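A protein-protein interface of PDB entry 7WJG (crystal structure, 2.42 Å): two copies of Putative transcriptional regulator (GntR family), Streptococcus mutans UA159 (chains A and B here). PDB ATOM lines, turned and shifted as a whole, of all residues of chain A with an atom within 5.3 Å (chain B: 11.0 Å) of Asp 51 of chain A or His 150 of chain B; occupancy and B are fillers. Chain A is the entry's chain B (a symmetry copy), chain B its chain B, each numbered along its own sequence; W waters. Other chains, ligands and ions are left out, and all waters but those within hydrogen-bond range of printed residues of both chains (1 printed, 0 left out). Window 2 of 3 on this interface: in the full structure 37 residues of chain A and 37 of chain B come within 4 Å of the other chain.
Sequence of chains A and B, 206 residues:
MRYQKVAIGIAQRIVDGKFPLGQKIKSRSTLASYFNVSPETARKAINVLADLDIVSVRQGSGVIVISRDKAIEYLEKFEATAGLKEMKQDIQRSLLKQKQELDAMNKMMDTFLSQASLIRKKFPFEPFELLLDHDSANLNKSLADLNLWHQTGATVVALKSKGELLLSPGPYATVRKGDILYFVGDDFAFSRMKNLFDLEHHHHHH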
ATOM      1  N   GLN A   4       8.249  20.601 -21.039  1.00  0.00           N
ATOM      2  CA  GLN A   4       7.155  19.826 -20.472  1.00  0.00           C
ATOM      3  C   GLN A   4       7.670  18.562 -19.781  1.00  0.00           C
ATOM      4  O   GLN A   4       7.201  18.210 -18.690  1.00  0.00           O
ATOM      5  CB  GLN A   4       6.148  19.499 -21.573  1.00  0.00           C
ATOM      6  CG  GLN A   4       4.832  18.946 -21.072  1.00  0.00           C
ATOM      7  CD  GLN A   4       4.873  17.437 -20.905  1.00  0.00           C
ATOM      8  OE1 GLN A   4       5.586  16.738 -21.631  1.00  0.00           O
ATOM      9  NE2 GLN A   4       4.112  16.927 -19.939  1.00  0.00           N
ATOM     10  N   ILE A  46       7.993  25.246 -14.754  1.00  0.00           N
ATOM     11  CA  ILE A  46       7.250  25.746 -13.604  1.00  0.00           C
ATOM     12  C   ILE A  46       5.885  26.293 -14.036  1.00  0.00           C
ATOM     13  O   ILE A  46       4.866  26.063 -13.374  1.00  0.00           O
ATOM     14  CB  ILE A  46       8.095  26.810 -12.881  1.00  0.00           C
ATOM     15  CG1 ILE A  46       9.301  26.168 -12.180  1.00  0.00           C
ATOM     16  CG2 ILE A  46       7.248  27.630 -11.920  1.00  0.00           C
ATOM     17  CD1 ILE A  46       8.907  25.193 -11.105  1.00  0.00           C
ATOM     18  N   ASN A  47       5.838  27.033 -15.144  1.00  0.00           N
ATOM     19  CA  ASN A  47       4.558  27.577 -15.579  1.00  0.00           C
ATOM     20  C   ASN A  47       3.562  26.466 -15.925  1.00  0.00           C
ATOM     21  O   ASN A  47       2.366  26.573 -15.608  1.00  0.00           O
ATOM     22  CB  ASN A  47       4.774  28.531 -16.756  1.00  0.00           C
ATOM     23  CG  ASN A  47       5.347  29.864 -16.306  1.00  0.00           C
ATOM     24  OD1 ASN A  47       5.400  30.152 -15.111  1.00  0.00           O
ATOM     25  ND2 ASN A  47       5.782  30.668 -17.241  1.00  0.00           N
ATOM     26  N   VAL A  48       4.033  25.388 -16.561  1.00  0.00           N
ATOM     27  CA  VAL A  48       3.163  24.240 -16.809  1.00  0.00           C
ATOM     28  C   VAL A  48       2.570  23.734 -15.496  1.00  0.00           C
ATOM     29  O   VAL A  48       1.356  23.523 -15.379  1.00  0.00           O
ATOM     30  CB  VAL A  48       3.926  23.131 -17.554  1.00  0.00           C
ATOM     31  CG1 VAL A  48       3.137  21.818 -17.530  1.00  0.00           C
ATOM     32  CG2 VAL A  48       4.191  23.554 -18.997  1.00  0.00           C
ATOM     33  N   LEU A  49       3.415  23.586 -14.475  1.00  0.00           N
ATOM     34  CA  LEU A  49       2.936  23.062 -13.200  1.00  0.00           C
ATOM     35  C   LEU A  49       1.994  24.034 -12.476  1.00  0.00           C
ATOM     36  O   LEU A  49       1.116  23.584 -11.732  1.00  0.00           O
ATOM     37  CB  LEU A  49       4.130  22.704 -12.311  1.00  0.00           C
ATOM     38  CG  LEU A  49       4.968  21.497 -12.732  1.00  0.00           C
ATOM     39  CD1 LEU A  49       5.956  21.119 -11.626  1.00  0.00           C
ATOM     40  CD2 LEU A  49       4.078  20.312 -13.067  1.00  0.00           C
ATOM     41  N   ALA A  50       2.187  25.355 -12.648  1.00  0.00           N
ATOM     42  CA  ALA A  50       1.302  26.341 -12.038  1.00  0.00           C
ATOM     43  C   ALA A  50      -0.083  26.319 -12.676  1.00  0.00           C
ATOM     44  O   ALA A  50      -1.100  26.392 -11.968  1.00  0.00           O
ATOM     45  CB  ALA A  50       1.904  27.742 -12.145  1.00  0.00           C
ATOM     46  N   ASP A  51      -0.141  26.251 -14.011  1.00  0.00           N
ATOM     47  CA  ASP A  51      -1.411  26.023 -14.681  1.00  0.00           C
ATOM     48  C   ASP A  51      -2.130  24.818 -14.090  1.00  0.00           C
ATOM     49  O   ASP A  51      -3.360  24.807 -14.003  1.00  0.00           O
ATOM     50  CB  ASP A  51      -1.199  25.813 -16.181  1.00  0.00           C
ATOM     51  CG  ASP A  51      -0.680  27.055 -16.877  1.00  0.00           C
ATOM     52  OD1 ASP A  51      -0.709  28.146 -16.282  1.00  0.00           O
ATOM     53  OD2 ASP A  51      -0.236  26.936 -18.025  1.00  0.00           O
ATOM     54  N   LEU A  52      -1.384  23.796 -13.675  1.00  0.00           N
ATOM     55  CA  LEU A  52      -2.014  22.584 -13.162  1.00  0.00           C
ATOM     56  C   LEU A  52      -2.303  22.673 -11.683  1.00  0.00           C
ATOM     57  O   LEU A  52      -2.704  21.668 -11.087  1.00  0.00           O
ATOM     58  CB  LEU A  52      -1.133  21.359 -13.418  1.00  0.00           C
ATOM     59  CG  LEU A  52      -0.960  20.950 -14.881  1.00  0.00           C
ATOM     60  CD1 LEU A  52       0.291  20.079 -14.978  1.00  0.00           C
ATOM     61  CD2 LEU A  52      -2.224  20.237 -15.441  1.00  0.00           C
ATOM     62  N   ASP A  53      -2.083  23.845 -11.098  1.00  0.00           N
ATOM     63  CA  ASP A  53      -2.267  24.101  -9.674  1.00  0.00           C
ATOM     64  C   ASP A  53      -1.441  23.160  -8.813  1.00  0.00           C
ATOM     65  O   ASP A  53      -1.780  22.899  -7.659  1.00  0.00           O
ATOM     66  CB  ASP A  53      -3.743  24.046  -9.299  1.00  0.00           C
ATOM     67  CG  ASP A  53      -4.505  25.215  -9.863  1.00  0.00           C
ATOM     68  OD1 ASP A  53      -3.922  26.328  -9.906  1.00  0.00           O
ATOM     69  OD2 ASP A  53      -5.671  25.038 -10.281  1.00  0.00           O
ATOM     70  N   TYR A  74      -0.947  14.052 -12.220  1.00  0.00           N
ATOM     71  CA  TYR A  74      -0.294  14.449 -13.453  1.00  0.00           C
ATOM     72  C   TYR A  74       0.629  13.342 -13.937  1.00  0.00           C
ATOM     73  O   TYR A  74       0.643  13.013 -15.129  1.00  0.00           O
ATOM     74  CB  TYR A  74       0.453  15.764 -13.251  1.00  0.00           C
ATOM     75  CG  TYR A  74       1.002  16.373 -14.515  1.00  0.00           C
ATOM     76  CD1 TYR A  74       0.190  16.557 -15.632  1.00  0.00           C
ATOM     77  CD2 TYR A  74       2.339  16.777 -14.589  1.00  0.00           C
ATOM     78  CE1 TYR A  74       0.692  17.122 -16.797  1.00  0.00           C
ATOM     79  CE2 TYR A  74       2.860  17.352 -15.747  1.00  0.00           C
ATOM     80  CZ  TYR A  74       2.033  17.520 -16.849  1.00  0.00           C
ATOM     81  OH  TYR A  74       2.545  18.079 -17.995  1.00  0.00           O
ATOM     82  N   PHE A  78       0.915  10.186 -17.682  1.00  0.00           N
ATOM     83  CA  PHE A  78       1.988   9.753 -18.556  1.00  0.00           C
ATOM     84  C   PHE A  78       2.468   8.334 -18.300  1.00  0.00           C
ATOM     85  O   PHE A  78       3.166   7.772 -19.150  1.00  0.00           O
ATOM     86  CB  PHE A  78       3.131  10.747 -18.445  1.00  0.00           C
ATOM     87  CG  PHE A  78       2.726  12.116 -18.885  1.00  0.00           C
ATOM     88  CD1 PHE A  78       2.604  12.401 -20.232  1.00  0.00           C
ATOM     89  CD2 PHE A  78       2.379  13.081 -17.963  1.00  0.00           C
ATOM     90  CE1 PHE A  78       2.185  13.645 -20.658  1.00  0.00           C
ATOM     91  CE2 PHE A  78       1.955  14.322 -18.378  1.00  0.00           C
ATOM     92  CZ  PHE A  78       1.853  14.600 -19.729  1.00  0.00           C
ATOM     93  N   SER B 142     -14.429  24.569 -19.620  1.00  0.00           N
ATOM     94  CA  SER B 142     -13.819  25.358 -20.670  1.00  0.00           C
ATOM     95  C   SER B 142     -12.437  24.806 -21.007  1.00  0.00           C
ATOM     96  O   SER B 142     -11.796  24.138 -20.194  1.00  0.00           O
ATOM     97  CB  SER B 142     -13.696  26.819 -20.240  1.00  0.00           C
ATOM     98  OG  SER B 142     -12.927  26.910 -19.053  1.00  0.00           O
ATOM     99  N   LEU B 143     -11.988  25.090 -22.231  1.00  0.00           N
ATOM    100  CA  LEU B 143     -10.660  24.660 -22.644  1.00  0.00           C
ATOM    101  C   LEU B 143      -9.593  25.254 -21.736  1.00  0.00           C
ATOM    102  O   LEU B 143      -8.620  24.576 -21.385  1.00  0.00           O
ATOM    103  CB  LEU B 143     -10.402  25.049 -24.102  1.00  0.00           C
ATOM    104  CG  LEU B 143     -11.250  24.332 -25.149  1.00  0.00           C
ATOM    105  CD1 LEU B 143     -10.896  24.805 -26.540  1.00  0.00           C
ATOM    106  CD2 LEU B 143     -11.066  22.817 -25.012  1.00  0.00           C
ATOM    107  N   ALA B 144      -9.765  26.520 -21.335  1.00  0.00           N
ATOM    108  CA  ALA B 144      -8.796  27.142 -20.438  1.00  0.00           C
ATOM    109  C   ALA B 144      -8.663  26.356 -19.137  1.00  0.00           C
ATOM    110  O   ALA B 144      -7.555  26.161 -18.632  1.00  0.00           O
ATOM    111  CB  ALA B 144      -9.194  28.589 -20.155  1.00  0.00           C
ATOM    112  N   ASP B 145      -9.779  25.889 -18.583  1.00  0.00           N
ATOM    113  CA  ASP B 145      -9.701  25.113 -17.352  1.00  0.00           C
ATOM    114  C   ASP B 145      -9.118  23.736 -17.588  1.00  0.00           C
ATOM    115  O   ASP B 145      -8.562  23.139 -16.663  1.00  0.00           O
ATOM    116  CB  ASP B 145     -11.083  24.941 -16.726  1.00  0.00           C
ATOM    117  CG  ASP B 145     -11.645  26.234 -16.142  1.00  0.00           C
ATOM    118  OD1 ASP B 145     -10.873  27.192 -15.863  1.00  0.00           O
ATOM    119  OD2 ASP B 145     -12.882  26.269 -15.963  1.00  0.00           O
ATOM    120  N   LEU B 146      -9.262  23.198 -18.799  1.00  0.00           N
ATOM    121  CA  LEU B 146      -8.967  21.787 -18.989  1.00  0.00           C
ATOM    122  C   LEU B 146      -7.476  21.465 -19.049  1.00  0.00           C
ATOM    123  O   LEU B 146      -7.117  20.319 -18.769  1.00  0.00           O
ATOM    124  CB  LEU B 146      -9.672  21.281 -20.240  1.00  0.00           C
ATOM    125  CG  LEU B 146     -11.153  21.010 -19.943  1.00  0.00           C
ATOM    126  CD1 LEU B 146     -11.923  20.815 -21.224  1.00  0.00           C
ATOM    127  CD2 LEU B 146     -11.335  19.812 -18.992  1.00  0.00           C
ATOM    128  N   ASN B 147      -6.610  22.437 -19.357  1.00  0.00           N
ATOM    129  CA  ASN B 147      -5.174  22.196 -19.534  1.00  0.00           C
ATOM    130  C   ASN B 147      -4.928  20.966 -20.403  1.00  0.00           C
ATOM    131  O   ASN B 147      -4.139  20.091 -20.057  1.00  0.00           O
ATOM    132  CB  ASN B 147      -4.457  22.018 -18.198  1.00  0.00           C
ATOM    133  CG  ASN B 147      -4.548  23.223 -17.315  1.00  0.00           C
ATOM    134  OD1 ASN B 147      -4.367  24.346 -17.767  1.00  0.00           O
ATOM    135  ND2 ASN B 147      -4.851  22.996 -16.023  1.00  0.00           N
ATOM    136  N   LEU B 148      -5.647  20.882 -21.525  1.00  0.00           N
ATOM    137  CA  LEU B 148      -5.536  19.692 -22.362  1.00  0.00           C
ATOM    138  C   LEU B 148      -4.103  19.502 -22.869  1.00  0.00           C
ATOM    139  O   LEU B 148      -3.578  18.382 -22.836  1.00  0.00           O
ATOM    140  CB  LEU B 148      -6.538  19.748 -23.526  1.00  0.00           C
ATOM    141  CG  LEU B 148      -8.047  19.752 -23.220  1.00  0.00           C
ATOM    142  CD1 LEU B 148      -8.896  19.802 -24.495  1.00  0.00           C
ATOM    143  CD2 LEU B 148      -8.458  18.542 -22.390  1.00  0.00           C
ATOM    144  N   TRP B 149      -3.444  20.574 -23.328  1.00  0.00           N
ATOM    145  CA  TRP B 149      -2.078  20.407 -23.827  1.00  0.00           C
ATOM    146  C   TRP B 149      -1.162  19.871 -22.736  1.00  0.00           C
ATOM    147  O   TRP B 149      -0.366  18.952 -22.963  1.00  0.00           O
ATOM    148  CB  TRP B 149      -1.496  21.720 -24.376  1.00  0.00           C
ATOM    149  CG  TRP B 149      -0.134  21.433 -24.992  1.00  0.00           C
ATOM    150  CD1 TRP B 149       0.105  21.009 -26.261  1.00  0.00           C
ATOM    151  CD2 TRP B 149       1.150  21.477 -24.337  1.00  0.00           C
ATOM    152  NE1 TRP B 149       1.451  20.787 -26.445  1.00  0.00           N
ATOM    153  CE2 TRP B 149       2.113  21.067 -25.283  1.00  0.00           C
ATOM    154  CE3 TRP B 149       1.572  21.818 -23.050  1.00  0.00           C
ATOM    155  CZ2 TRP B 149       3.481  21.005 -24.987  1.00  0.00           C
ATOM    156  CZ3 TRP B 149       2.929  21.742 -22.748  1.00  0.00           C
ATOM    157  CH2 TRP B 149       3.868  21.345 -23.718  1.00  0.00           C
ATOM    158  N   HIS B 150      -1.243  20.468 -21.547  1.00  0.00           N
ATOM    159  CA  HIS B 150      -0.413  20.042 -20.429  1.00  0.00           C
ATOM    160  C   HIS B 150      -0.535  18.542 -20.173  1.00  0.00           C
ATOM    161  O   HIS B 150       0.468  17.857 -19.911  1.00  0.00           O
ATOM    162  CB  HIS B 150      -0.810  20.815 -19.171  1.00  0.00           C
ATOM    163  CG  HIS B 150      -0.803  22.304 -19.331  1.00  0.00           C
ATOM    164  ND1 HIS B 150      -1.641  22.975 -20.204  1.00  0.00           N
ATOM    165  CD2 HIS B 150      -0.075  23.257 -18.699  1.00  0.00           C
ATOM    166  CE1 HIS B 150      -1.427  24.277 -20.097  1.00  0.00           C
ATOM    167  NE2 HIS B 150      -0.483  24.473 -19.191  1.00  0.00           N
ATOM    168  N   GLN B 151      -1.756  18.016 -20.264  1.00  0.00           N
ATOM    169  CA  GLN B 151      -2.052  16.649 -19.855  1.00  0.00           C
ATOM    170  C   GLN B 151      -2.012  15.648 -20.999  1.00  0.00           C
ATOM    171  O   GLN B 151      -2.136  14.444 -20.754  1.00  0.00           O
ATOM    172  CB  GLN B 151      -3.430  16.600 -19.186  1.00  0.00           C
ATOM    173  CG  GLN B 151      -3.492  17.406 -17.916  1.00  0.00           C
ATOM    174  CD  GLN B 151      -4.830  17.325 -17.273  1.00  0.00           C
ATOM    175  OE1 GLN B 151      -5.744  18.049 -17.650  1.00  0.00           O
ATOM    176  NE2 GLN B 151      -4.973  16.436 -16.303  1.00  0.00           N
ATOM    177  N   THR B 152      -1.868  16.105 -22.238  1.00  0.00           N
ATOM    178  CA  THR B 152      -1.936  15.184 -23.365  1.00  0.00           C
ATOM    179  C   THR B 152      -0.915  15.453 -24.459  1.00  0.00           C
ATOM    180  O   THR B 152      -0.605  14.521 -25.207  1.00  0.00           O
ATOM    181  CB  THR B 152      -3.336  15.207 -24.012  1.00  0.00           C
ATOM    182  OG1 THR B 152      -3.462  16.398 -24.797  1.00  0.00           O
ATOM    183  CG2 THR B 152      -4.479  15.136 -22.966  1.00  0.00           C
ATOM    184  N   GLY B 153      -0.404  16.678 -24.604  1.00  0.00           N
ATOM    185  CA  GLY B 153       0.325  17.081 -25.788  1.00  0.00           C
ATOM    186  C   GLY B 153      -0.527  17.377 -27.005  1.00  0.00           C
ATOM    187  O   GLY B 153       0.025  17.570 -28.094  1.00  0.00           O
ATOM    188  N   ALA B 154      -1.852  17.424 -26.863  1.00  0.00           N
ATOM    189  CA  ALA B 154      -2.737  17.742 -27.975  1.00  0.00           C
ATOM    190  C   ALA B 154      -2.989  19.242 -28.050  1.00  0.00           C
ATOM    191  O   ALA B 154      -3.036  19.935 -27.030  1.00  0.00           O
ATOM    192  CB  ALA B 154      -4.060  16.996 -27.834  1.00  0.00           C
ATOM    193  N   THR B 155      -3.128  19.753 -29.270  1.00  0.00           N
ATOM    194  CA  THR B 155      -3.641  21.104 -29.466  1.00  0.00           C
ATOM    195  C   THR B 155      -4.989  21.023 -30.162  1.00  0.00           C
ATOM    196  O   THR B 155      -5.069  20.630 -31.326  1.00  0.00           O
ATOM    197  CB  THR B 155      -2.667  21.968 -30.250  1.00  0.00           C
ATOM    198  OG1 THR B 155      -1.433  21.973 -29.546  1.00  0.00           O
ATOM    199  CG2 THR B 155      -3.180  23.402 -30.332  1.00  0.00           C
ATOM    200  N   VAL B 156      -6.045  21.393 -29.438  1.00  0.00           N
ATOM    201  CA  VAL B 156      -7.384  21.444 -30.013  1.00  0.00           C
ATOM    202  C   VAL B 156      -7.419  22.492 -31.115  1.00  0.00           C
ATOM    203  O   VAL B 156      -6.979  23.634 -30.923  1.00  0.00           O
ATOM    204  CB  VAL B 156      -8.400  21.755 -28.907  1.00  0.00           C
ATOM    205  CG1 VAL B 156      -9.813  22.019 -29.491  1.00  0.00           C
ATOM    206  CG2 VAL B 156      -8.408  20.624 -27.905  1.00  0.00           C
ATOM    207  N   PRO B 171     -10.121  29.696 -25.650  1.00  0.00           N
ATOM    208  CA  PRO B 171     -10.129  29.212 -24.251  1.00  0.00           C
ATOM    209  C   PRO B 171     -11.484  29.304 -23.557  1.00  0.00           C
ATOM    210  O   PRO B 171     -11.704  28.578 -22.577  1.00  0.00           O
ATOM    211  CB  PRO B 171      -9.091  30.104 -23.555  1.00  0.00           C
ATOM    212  CG  PRO B 171      -8.859  31.276 -24.485  1.00  0.00           C
ATOM    213  CD  PRO B 171      -9.241  30.857 -25.868  1.00  0.00           C
ATOM    214  N   VAL B 184      -4.502  18.318 -32.945  1.00  0.00           N
ATOM    215  CA  VAL B 184      -3.279  17.839 -33.578  1.00  0.00           C
ATOM    216  C   VAL B 184      -2.252  17.465 -32.515  1.00  0.00           C
ATOM    217  O   VAL B 184      -2.269  17.955 -31.381  1.00  0.00           O
ATOM    218  CB  VAL B 184      -2.692  18.861 -34.584  1.00  0.00           C
ATOM    219  CG1 VAL B 184      -3.697  19.108 -35.719  1.00  0.00           C
ATOM    220  CG2 VAL B 184      -2.283  20.169 -33.887  1.00  0.00           C
ATOM    221  N   PHE B 188       0.877   9.544 -29.165  1.00  0.00           N
ATOM    222  CA  PHE B 188       0.716   9.639 -27.717  1.00  0.00           C
ATOM    223  C   PHE B 188      -0.359  10.644 -27.352  1.00  0.00           C
ATOM    224  O   PHE B 188      -1.165  10.402 -26.446  1.00  0.00           O
ATOM    225  CB  PHE B 188       2.026  10.035 -27.054  1.00  0.00           C
ATOM    226  CG  PHE B 188       3.091   9.010 -27.171  1.00  0.00           C
ATOM    227  CD1 PHE B 188       3.218   8.013 -26.221  1.00  0.00           C
ATOM    228  CD2 PHE B 188       3.970   9.042 -28.229  1.00  0.00           C
ATOM    229  CE1 PHE B 188       4.211   7.067 -26.326  1.00  0.00           C
ATOM    230  CE2 PHE B 188       4.961   8.100 -28.346  1.00  0.00           C
ATOM    231  CZ  PHE B 188       5.088   7.118 -27.389  1.00  0.00           C
ATOM    232  N   ALA B 189      -0.394  11.781 -28.044  1.00  0.00           N
ATOM    233  CA  ALA B 189      -1.403  12.775 -27.704  1.00  0.00           C
ATOM    234  C   ALA B 189      -2.811  12.253 -27.976  1.00  0.00           C
ATOM    235  O   ALA B 189      -3.746  12.583 -27.238  1.00  0.00           O
ATOM    236  CB  ALA B 189      -1.135  14.082 -28.452  1.00  0.00           C
ATOM    237  N   ARG B 192      -3.681   9.969 -25.018  1.00  0.00           N
ATOM    238  CA  ARG B 192      -3.832  10.705 -23.772  1.00  0.00           C
ATOM    239  C   ARG B 192      -5.120  11.516 -23.768  1.00  0.00           C
ATOM    240  O   ARG B 192      -5.767  11.629 -22.720  1.00  0.00           O
ATOM    241  CB  ARG B 192      -2.597  11.575 -23.531  1.00  0.00           C
ATOM    242  CG  ARG B 192      -1.448  10.774 -22.933  1.00  0.00           C
ATOM    243  CD  ARG B 192      -0.064  11.342 -23.264  1.00  0.00           C
ATOM    244  NE  ARG B 192       0.985  10.431 -22.810  1.00  0.00           N
ATOM    245  CZ  ARG B 192       2.264  10.519 -23.161  1.00  0.00           C
ATOM    246  NH1 ARG B 192       2.676  11.486 -23.980  1.00  0.00           N
ATOM    247  NH2 ARG B 192       3.138   9.640 -22.686  1.00  0.00           N
ATOM    248  N   MET B 193      -5.538  12.045 -24.926  1.00  0.00           N
ATOM    249  CA  MET B 193      -6.857  12.669 -24.992  1.00  0.00           C
ATOM    250  C   MET B 193      -7.933  11.652 -24.668  1.00  0.00           C
ATOM    251  O   MET B 193      -8.846  11.928 -23.877  1.00  0.00           O
ATOM    252  CB  MET B 193      -7.118  13.287 -26.376  1.00  0.00           C
ATOM    253  CG  MET B 193      -6.458  14.642 -26.604  1.00  0.00           C
ATOM    254  SD  MET B 193      -7.146  15.980 -25.599  1.00  0.00           S
ATOM    255  CE  MET B 193      -8.796  16.115 -26.299  1.00  0.00           C
ATOM    256  N   LEU B 196      -8.196  10.801 -21.024  1.00  0.00           N
ATOM    257  CA  LEU B 196      -8.628  11.952 -20.248  1.00  0.00           C
ATOM    258  C   LEU B 196     -10.144  12.088 -20.213  1.00  0.00           C
ATOM    259  O   LEU B 196     -10.699  12.518 -19.200  1.00  0.00           O
ATOM    260  CB  LEU B 196      -7.978  13.211 -20.825  1.00  0.00           C
ATOM    261  CG  LEU B 196      -8.172  14.457 -19.977  1.00  0.00           C
ATOM    262  CD1 LEU B 196      -7.512  14.252 -18.596  1.00  0.00           C
ATOM    263  CD2 LEU B 196      -7.609  15.641 -20.685  1.00  0.00           C
HETATM  264  O   HOH W   1       0.405   7.940 -21.149  1.00  0.00           O
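No position is printed for both chains. Of the 10 pairs that touch across the chains among the printed residues, none has its exchanged pair printed and touching as well.
Of chain B, only Asn 147 and His 150 come within 4 Å of Asp 51 of chain A. His 150 of chain B touches just these residues of chain A: Gln 4, Val 48, Asp 51, Tyr 74 and Phe 78. Val 48 of chain A touches one residue of chain B. No residue of chain B comes within 4 Å of Ala 50 of chain A. Of chain B, only Asn 147 (3.9 Å) and Gln 151 (3.97 Å) come within 4 Å of Leu 52 of chain A. No residue of chain B comes within 4 Å of Asp 53 of chain A. Printed residues of chain A within 4 Å of Arg 192 of chain B: Phe 78 (3.5 Å). Of the printed residues of chain A, Asn 147 of chain B touches Asp 51 and Leu 52. Of the printed residues of chain B, Tyr 74 of chain A touches His 150. Of the printed residues of chain B, Gln 4 of chain A touches Trp 149 (3.6 Å) and His 150 (3.8 Å). The nearest printed residue of chain A that does not touch Trp 149 of chain B is Val 48 of chain A (4.4 Å).
Of the 11 printed residues of chain A, 6 touch a printed residue of chain B. Of the 22 printed residues of chain B, 5 touch a printed residue of chain A. Among the printed residues, 10 pairs touch across the chains. Among the printed residues, no Asp or Glu carboxylate lies within 4 Å of a Lys or Arg side-chain nitrogen of the other chain.
Water W1 bridges the guanidinium group (NE) of Arg 192 of chain B (3.0 Å) and the backbone carbonyl oxygen (O) of Phe 78 of chain A (3.4 Å).
CB of Gln 4 of chain A touches CH2 of Trp 149 of chain B, 3.6 Å away. NE2 of Gln 4 of chain A touches O of His 150 of chain B, at 3.8 Å. Val 48 of chain A touches His 150 of chain B (O to CD2, 3.6 Å). CD2 of Leu 52 of chain A touches ND2 of Asn 147 of chain B (3.9 Å). CD2 of Leu 52 of chain A touches CG of Gln 151 of chain B (3.97 Å). His 150 of chain B touches Phe 78 of chain A. CD1 of Phe 78 of chain A touches CZ of Arg 192 of chain B, at 3.5 Å.
The side-chain amide nitrogen of Asn 147 of chain B lies within hydrogen-bond range of the backbone carbonyl oxygen of Asp 51 of chain A (3.1 Å). The side-chain carboxylate of Asp 51 of chain A is in hydrogen-bond range of a ring nitrogen (NE2) of His 150 of chain B, 2.7 Å away. OH of Tyr 74 of chain A lies within hydrogen-bond range of O of His 150 of chain B (2.8 Å).
O of Leu 146 of chain B sits close to OE1 of Gln 151 of chain B, 2.9 Å away. OH of Tyr 74 of chain A sits at hydrogen-bond distance from NE2 of Gln 4 of chain A, 2.7 Å away.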
